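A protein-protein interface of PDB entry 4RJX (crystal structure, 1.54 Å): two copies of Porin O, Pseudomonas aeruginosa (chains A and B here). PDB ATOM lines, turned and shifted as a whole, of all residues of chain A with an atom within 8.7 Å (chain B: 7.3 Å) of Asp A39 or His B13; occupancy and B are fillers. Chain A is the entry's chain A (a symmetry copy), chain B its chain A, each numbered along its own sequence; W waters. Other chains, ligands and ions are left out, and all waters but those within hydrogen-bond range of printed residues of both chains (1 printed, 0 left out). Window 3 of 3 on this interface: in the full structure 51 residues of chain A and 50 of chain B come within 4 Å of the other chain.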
ATOM      1  N   GLY A  22      14.342   5.419  16.664  1.00  0.00           N
ATOM      2  CA  GLY A  22      13.500   6.100  15.696  1.00  0.00           C
ATOM      3  C   GLY A  22      14.240   7.205  14.965  1.00  0.00           C
ATOM      4  O   GLY A  22      15.447   7.116  14.736  1.00  0.00           O
ATOM      5  N   ALA A  23      13.509   8.259  14.614  1.00  0.00           N
ATOM      6  CA  ALA A  23      14.077   9.412  13.928  1.00  0.00           C
ATOM      7  C   ALA A  23      15.153  10.090  14.766  1.00  0.00           C
ATOM      8  O   ALA A  23      15.069  10.083  16.005  1.00  0.00           O
ATOM      9  CB  ALA A  23      12.979  10.406  13.583  1.00  0.00           C
ATOM     10  N   ASP A  24      16.150  10.672  14.093  1.00  0.00           N
ATOM     11  CA  ASP A  24      17.219  11.414  14.762  1.00  0.00           C
ATOM     12  C   ASP A  24      16.673  12.358  15.836  1.00  0.00           C
ATOM     13  O   ASP A  24      15.650  13.010  15.638  1.00  0.00           O
ATOM     14  CB  ASP A  24      18.047  12.239  13.767  1.00  0.00           C
ATOM     15  CG  ASP A  24      18.868  11.381  12.807  1.00  0.00           C
ATOM     16  OD1 ASP A  24      19.035  10.152  13.023  1.00  0.00           O
ATOM     17  OD2 ASP A  24      19.384  11.966  11.828  1.00  0.00           O
ATOM     18  N   ILE A  25      17.385  12.424  16.953  1.00  0.00           N
ATOM     19  CA  ILE A  25      17.007  13.251  18.089  1.00  0.00           C
ATOM     20  C   ILE A  25      18.073  14.304  18.364  1.00  0.00           C
ATOM     21  O   ILE A  25      19.271  14.043  18.218  1.00  0.00           O
ATOM     22  CB  ILE A  25      16.787  12.384  19.349  1.00  0.00           C
ATOM     23  CG1 ILE A  25      15.412  11.714  19.298  1.00  0.00           C
ATOM     24  CG2 ILE A  25      16.896  13.210  20.633  1.00  0.00           C
ATOM     25  CD1 ILE A  25      15.148  10.769  20.467  1.00  0.00           C
ATOM     26  N   VAL A  26      17.620  15.500  18.726  1.00  0.00           N
ATOM     27  CA  VAL A  26      18.486  16.552  19.234  1.00  0.00           C
ATOM     28  C   VAL A  26      18.129  16.806  20.685  1.00  0.00           C
ATOM     29  O   VAL A  26      16.958  16.946  21.021  1.00  0.00           O
ATOM     30  CB  VAL A  26      18.341  17.849  18.427  1.00  0.00           C
ATOM     31  CG1 VAL A  26      19.131  18.974  19.075  1.00  0.00           C
ATOM     32  CG2 VAL A  26      18.821  17.623  16.998  1.00  0.00           C
ATOM     33  N   ALA A  36      13.973  16.282  21.189  1.00  0.00           N
ATOM     34  CA  ALA A  36      13.053  16.388  20.064  1.00  0.00           C
ATOM     35  C   ALA A  36      13.564  15.632  18.851  1.00  0.00           C
ATOM     36  O   ALA A  36      14.771  15.608  18.601  1.00  0.00           O
ATOM     37  CB  ALA A  36      12.829  17.850  19.704  1.00  0.00           C
ATOM     38  N   THR A  37      12.657  15.020  18.088  1.00  0.00           N
ATOM     39  CA  THR A  37      13.064  14.409  16.821  1.00  0.00           C
ATOM     40  C   THR A  37      13.210  15.488  15.747  1.00  0.00           C
ATOM     41  O   THR A  37      12.490  16.478  15.743  1.00  0.00           O
ATOM     42  CB  THR A  37      12.071  13.321  16.351  1.00  0.00           C
ATOM     43  OG1 THR A  37      10.750  13.875  16.236  1.00  0.00           O
ATOM     44  CG2 THR A  37      12.047  12.153  17.329  1.00  0.00           C
ATOM     45  N   THR A  38      14.151  15.297  14.826  1.00  0.00           N
ATOM     46  CA  THR A  38      14.444  16.340  13.847  1.00  0.00           C
ATOM     47  C   THR A  38      13.375  16.454  12.766  1.00  0.00           C
ATOM     48  O   THR A  38      13.320  17.448  12.041  1.00  0.00           O
ATOM     49  CB  THR A  38      15.812  16.107  13.182  1.00  0.00           C
ATOM     50  OG1 THR A  38      15.817  14.837  12.516  1.00  0.00           O
ATOM     51  CG2 THR A  38      16.893  16.124  14.241  1.00  0.00           C
ATOM     52  N   ASP A  39      12.520  15.445  12.659  1.00  0.00           N
ATOM     53  CA  ASP A  39      11.398  15.504  11.728  1.00  0.00           C
ATOM     54  C   ASP A  39      10.180  16.227  12.329  1.00  0.00           C
ATOM     55  O   ASP A  39       9.108  16.241  11.721  1.00  0.00           O
ATOM     56  CB  ASP A  39      10.999  14.098  11.284  1.00  0.00           C
ATOM     57  CG  ASP A  39      10.576  13.209  12.437  1.00  0.00           C
ATOM     58  OD1 ASP A  39      10.381  13.705  13.575  1.00  0.00           O
ATOM     59  OD2 ASP A  39      10.418  11.997  12.197  1.00  0.00           O
ATOM     60  N   LYS A  40      10.354  16.784  13.528  1.00  0.00           N
ATOM     61  CA  LYS A  40       9.313  17.563  14.220  1.00  0.00           C
ATOM     62  C   LYS A  40       8.085  16.759  14.671  1.00  0.00           C
ATOM     63  O   LYS A  40       7.067  17.344  15.068  1.00  0.00           O
ATOM     64  CB  LYS A  40       8.848  18.731  13.337  1.00  0.00           C
ATOM     65  CG  LYS A  40       9.953  19.715  12.988  1.00  0.00           C
ATOM     66  N   GLU A  41       8.171  15.438  14.652  1.00  0.00           N
ATOM     67  CA  GLU A  41       7.022  14.615  15.022  1.00  0.00           C
ATOM     68  C   GLU A  41       6.821  14.529  16.539  1.00  0.00           C
ATOM     69  O   GLU A  41       5.685  14.536  17.027  1.00  0.00           O
ATOM     70  CB  GLU A  41       7.165  13.203  14.446  1.00  0.00           C
ATOM     71  CG  GLU A  41       6.945  13.100  12.947  1.00  0.00           C
ATOM     72  CD  GLU A  41       5.475  13.017  12.569  1.00  0.00           C
ATOM     73  OE1 GLU A  41       4.673  12.507  13.380  1.00  0.00           O
ATOM     74  OE2 GLU A  41       5.127  13.452  11.449  1.00  0.00           O
ATOM     75  N   PHE A  42       7.921  14.452  17.286  1.00  0.00           N
ATOM     76  CA  PHE A  42       7.845  14.251  18.729  1.00  0.00           C
ATOM     77  C   PHE A  42       8.808  15.168  19.470  1.00  0.00           C
ATOM     78  O   PHE A  42       9.915  15.438  18.997  1.00  0.00           O
ATOM     79  CB  PHE A  42       8.156  12.795  19.103  1.00  0.00           C
ATOM     80  CG  PHE A  42       7.224  11.796  18.499  1.00  0.00           C
ATOM     81  CD1 PHE A  42       5.961  11.598  19.028  1.00  0.00           C
ATOM     82  CD2 PHE A  42       7.622  11.036  17.409  1.00  0.00           C
ATOM     83  CE1 PHE A  42       5.093  10.672  18.466  1.00  0.00           C
ATOM     84  CE2 PHE A  42       6.761  10.105  16.852  1.00  0.00           C
ATOM     85  CZ  PHE A  42       5.502   9.923  17.380  1.00  0.00           C
ATOM     86  N   SER A  43       8.397  15.637  20.644  1.00  0.00           N
ATOM     87  CA  SER A  43       9.291  16.433  21.467  1.00  0.00           C
ATOM     88  C   SER A  43       8.849  16.412  22.924  1.00  0.00           C
ATOM     89  O   SER A  43       7.687  16.110  23.236  1.00  0.00           O
ATOM     90  CB  SER A  43       9.353  17.878  20.959  1.00  0.00           C
ATOM     91  OG  SER A  43       8.183  18.591  21.320  1.00  0.00           O
ATOM     92  N   THR A  83       5.203  17.325  22.290  1.00  0.00           N
ATOM     93  CA  THR A  83       4.517  17.185  21.015  1.00  0.00           C
ATOM     94  C   THR A  83       4.475  15.712  20.643  1.00  0.00           C
ATOM     95  O   THR A  83       5.443  14.983  20.890  1.00  0.00           O
ATOM     96  CB  THR A  83       5.244  17.969  19.900  1.00  0.00           C
ATOM     97  OG1 THR A  83       5.333  19.350  20.279  1.00  0.00           O
ATOM     98  CG2 THR A  83       4.503  17.849  18.571  1.00  0.00           C
ATOM     99  N   TYR A  85       3.032  13.146  17.268  1.00  0.00           N
ATOM    100  CA  TYR A  85       2.432  13.050  15.937  1.00  0.00           C
ATOM    101  C   TYR A  85       2.297  14.431  15.295  1.00  0.00           C
ATOM    102  O   TYR A  85       1.318  14.731  14.615  1.00  0.00           O
ATOM    103  CB  TYR A  85       1.097  12.299  16.019  1.00  0.00           C
ATOM    104  CG  TYR A  85       1.327  10.913  16.567  1.00  0.00           C
ATOM    105  CD1 TYR A  85       1.795   9.897  15.738  1.00  0.00           C
ATOM    106  CD2 TYR A  85       1.163  10.634  17.920  1.00  0.00           C
ATOM    107  CE1 TYR A  85       2.047   8.639  16.228  1.00  0.00           C
ATOM    108  CE2 TYR A  85       1.420   9.365  18.422  1.00  0.00           C
ATOM    109  CZ  TYR A  85       1.863   8.376  17.563  1.00  0.00           C
ATOM    110  OH  TYR A  85       2.133   7.103  18.013  1.00  0.00           O
ATOM    111  N   LYS A  86       3.320  15.247  15.540  1.00  0.00           N
ATOM    112  CA  LYS A  86       3.513  16.575  14.951  1.00  0.00           C
ATOM    113  C   LYS A  86       2.520  17.655  15.420  1.00  0.00           C
ATOM    114  O   LYS A  86       2.933  18.771  15.741  1.00  0.00           O
ATOM    115  CB  LYS A  86       3.479  16.479  13.419  1.00  0.00           C
ATOM    116  CG  LYS A  86       3.739  17.792  12.708  1.00  0.00           C
ATOM    117  CD  LYS A  86       3.760  17.598  11.193  1.00  0.00           C
ATOM    118  CE  LYS A  86       3.830  18.932  10.468  1.00  0.00           C
ATOM    119  NZ  LYS A  86       4.968  19.764  10.946  1.00  0.00           N
ATOM    120  N   HIS B  10       5.154  10.584   0.698  1.00  0.00           N
ATOM    121  CA  HIS B  10       5.871   9.790   1.685  1.00  0.00           C
ATOM    122  C   HIS B  10       7.297  10.299   1.792  1.00  0.00           C
ATOM    123  O   HIS B  10       7.816  10.903   0.855  1.00  0.00           O
ATOM    124  CB  HIS B  10       5.845   8.301   1.320  1.00  0.00           C
ATOM    125  CG  HIS B  10       6.964   7.873   0.421  1.00  0.00           C
ATOM    126  ND1 HIS B  10       7.024   8.213  -0.913  1.00  0.00           N
ATOM    127  CD2 HIS B  10       8.061   7.115   0.664  1.00  0.00           C
ATOM    128  CE1 HIS B  10       8.111   7.689  -1.452  1.00  0.00           C
ATOM    129  NE2 HIS B  10       8.756   7.017  -0.515  1.00  0.00           N
ATOM    130  N   HIS B  11       7.927  10.047   2.933  1.00  0.00           N
ATOM    131  CA  HIS B  11       9.262  10.562   3.195  1.00  0.00           C
ATOM    132  C   HIS B  11      10.213   9.468   3.672  1.00  0.00           C
ATOM    133  O   HIS B  11       9.789   8.460   4.237  1.00  0.00           O
ATOM    134  CB  HIS B  11       9.196  11.687   4.231  1.00  0.00           C
ATOM    135  CG  HIS B  11       8.239  12.781   3.868  1.00  0.00           C
ATOM    136  ND1 HIS B  11       8.529  13.736   2.917  1.00  0.00           N
ATOM    137  CD2 HIS B  11       6.996  13.065   4.319  1.00  0.00           C
ATOM    138  CE1 HIS B  11       7.506  14.563   2.801  1.00  0.00           C
ATOM    139  NE2 HIS B  11       6.562  14.177   3.641  1.00  0.00           N
ATOM    140  N   HIS B  12      11.503   9.673   3.413  1.00  0.00           N
ATOM    141  CA  HIS B  12      12.559   8.845   3.975  1.00  0.00           C
ATOM    142  C   HIS B  12      13.209   9.632   5.106  1.00  0.00           C
ATOM    143  O   HIS B  12      13.854  10.648   4.861  1.00  0.00           O
ATOM    144  CB  HIS B  12      13.604   8.475   2.917  1.00  0.00           C
ATOM    145  CG  HIS B  12      13.062   7.704   1.750  1.00  0.00           C
ATOM    146  ND1 HIS B  12      13.813   7.448   0.621  1.00  0.00           N
ATOM    147  CD2 HIS B  12      11.853   7.130   1.533  1.00  0.00           C
ATOM    148  CE1 HIS B  12      13.089   6.754  -0.239  1.00  0.00           C
ATOM    149  NE2 HIS B  12      11.897   6.546   0.289  1.00  0.00           N
ATOM    150  N   HIS B  13      13.038   9.180   6.341  1.00  0.00           N
ATOM    151  CA  HIS B  13      13.549   9.937   7.478  1.00  0.00           C
ATOM    152  C   HIS B  13      14.872   9.384   8.001  1.00  0.00           C
ATOM    153  O   HIS B  13      15.061   8.170   8.094  1.00  0.00           O
ATOM    154  CB  HIS B  13      12.510   9.972   8.603  1.00  0.00           C
ATOM    155  CG  HIS B  13      11.331  10.849   8.308  1.00  0.00           C
ATOM    156  ND1 HIS B  13      10.052  10.355   8.156  1.00  0.00           N
ATOM    157  CD2 HIS B  13      11.241  12.189   8.127  1.00  0.00           C
ATOM    158  CE1 HIS B  13       9.224  11.353   7.901  1.00  0.00           C
ATOM    159  NE2 HIS B  13       9.920  12.476   7.877  1.00  0.00           N
ATOM    160  N   LEU B  14      15.788  10.293   8.331  1.00  0.00           N
ATOM    161  CA  LEU B  14      17.069   9.932   8.927  1.00  0.00           C
ATOM    162  C   LEU B  14      16.853   9.428  10.344  1.00  0.00           C
ATOM    163  O   LEU B  14      16.195  10.094  11.148  1.00  0.00           O
ATOM    164  CB  LEU B  14      18.020  11.129   8.935  1.00  0.00           C
ATOM    165  CG  LEU B  14      18.446  11.668   7.569  1.00  0.00           C
ATOM    166  CD1 LEU B  14      18.291  13.176   7.518  1.00  0.00           C
ATOM    167  CD2 LEU B  14      19.881  11.263   7.281  1.00  0.00           C
ATOM    168  N   GLU B  15      17.413   8.263  10.653  1.00  0.00           N
ATOM    169  CA  GLU B  15      17.160   7.626  11.940  1.00  0.00           C
ATOM    170  C   GLU B  15      18.429   7.267  12.713  1.00  0.00           C
ATOM    171  O   GLU B  15      19.502   7.079  12.132  1.00  0.00           O
ATOM    172  CB  GLU B  15      16.320   6.363  11.736  1.00  0.00           C
ATOM    173  CG  GLU B  15      14.900   6.631  11.266  1.00  0.00           C
ATOM    174  CD  GLU B  15      14.107   5.357  11.055  1.00  0.00           C
ATOM    175  OE1 GLU B  15      12.936   5.305  11.491  1.00  0.00           O
ATOM    176  OE2 GLU B  15      14.652   4.410  10.451  1.00  0.00           O
ATOM    177  N   GLY B  16      18.297   7.192  14.035  1.00  0.00           N
ATOM    178  CA  GLY B  16      19.325   6.586  14.853  1.00  0.00           C
ATOM    179  C   GLY B  16      20.285   7.475  15.620  1.00  0.00           C
ATOM    180  O   GLY B  16      20.818   7.026  16.627  1.00  0.00           O
HETATM  181  O   HOH W   1      14.566  12.432  11.053  1.00  0.00           O
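The backbone NH (N) of Gly B16 sits at hydrogen-bond distance from the side-chain carboxylate (OD1) of Asp A24 (3.2 Å).
The backbone NH (N) of Gly B16 sits at hydrogen-bond distance from the backbone carbonyl oxygen (O) of Gly A22.
O of Leu B14 sits at hydrogen-bond distance from N of Asp A24 (3.0 Å).
N of Glu B15 sits close to OD1 of Asp A24 (3.4 Å).
The backbone carbonyl oxygen (O) of Asp A24 is in hydrogen-bond range of the backbone NH (N) of Thr A38, at 2.9 Å.
The backbone NH (N) of Glu A41 is in hydrogen-bond range of the side-chain carboxylate (OD1) of Asp A39 (3.0 Å).
The side-chain hydroxyl (OG1) of Thr A37 is in hydrogen-bond range of the side-chain carboxylate (OD1) of Asp A39, 2.7 Å away.
Among the printed residues, pairs that only touch across the chains: Gly A22 with Glu B15, Ala A23 with Leu B14, Asp A39 with His B13 and Ala A23 with Glu B15.
Of the printed residues of chain B, Gly A22 touches Glu B15 (3.2 Å) and Gly B16 (2.9 Å).
Of chain B, only His B13 comes within 4 Å of Asp A39.
Of the printed residues of chain A, Leu B14 touches Ala A23 and Asp A24.
Printed residues of chain A within 4 Å of Glu B15: Gly A22, Ala A23 and Asp A24.
Printed residues of chain A within 4 Å of Gly B16: Gly A22 (2.9 Å) and Asp A24 (3.2 Å).
The nearest residue of chain A that does not touch His B13 is Ala A23 (5.0 Å).
The nearest printed residue of chain B that does not touch Asp A24 is His B13 (6.4 Å).
Of the 7 printed residues of chain B, 4 touch a printed residue of chain A.
Printed residues of chain B that touch a printed residue of chain A: His B13, Leu B14, Glu B15 and Gly B16.
Hydrophobic or aromatic side chains of chain B within 4 Å of the printed part of chain A: His B13 and Leu B14.
Along chain B the printed residues that touch a printed residue of chain A span positions 13 to 16.
Among the printed residues, 8 pairs touch across the chains.
Among the printed residues, no Asp or Glu carboxylate lies within 4 Å of a Lys or Arg side-chain nitrogen of the other chain.
No position is printed for both chains.
Of the 8 pairs that touch across the chains among the printed residues, none has its exchanged pair printed and touching as well.
Water W1 lies within hydrogen-bond range of the backbone carbonyl oxygen of Leu B14 (2.9 Å) and the side-chain hydroxyl of Thr A38 (3.1 Å).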
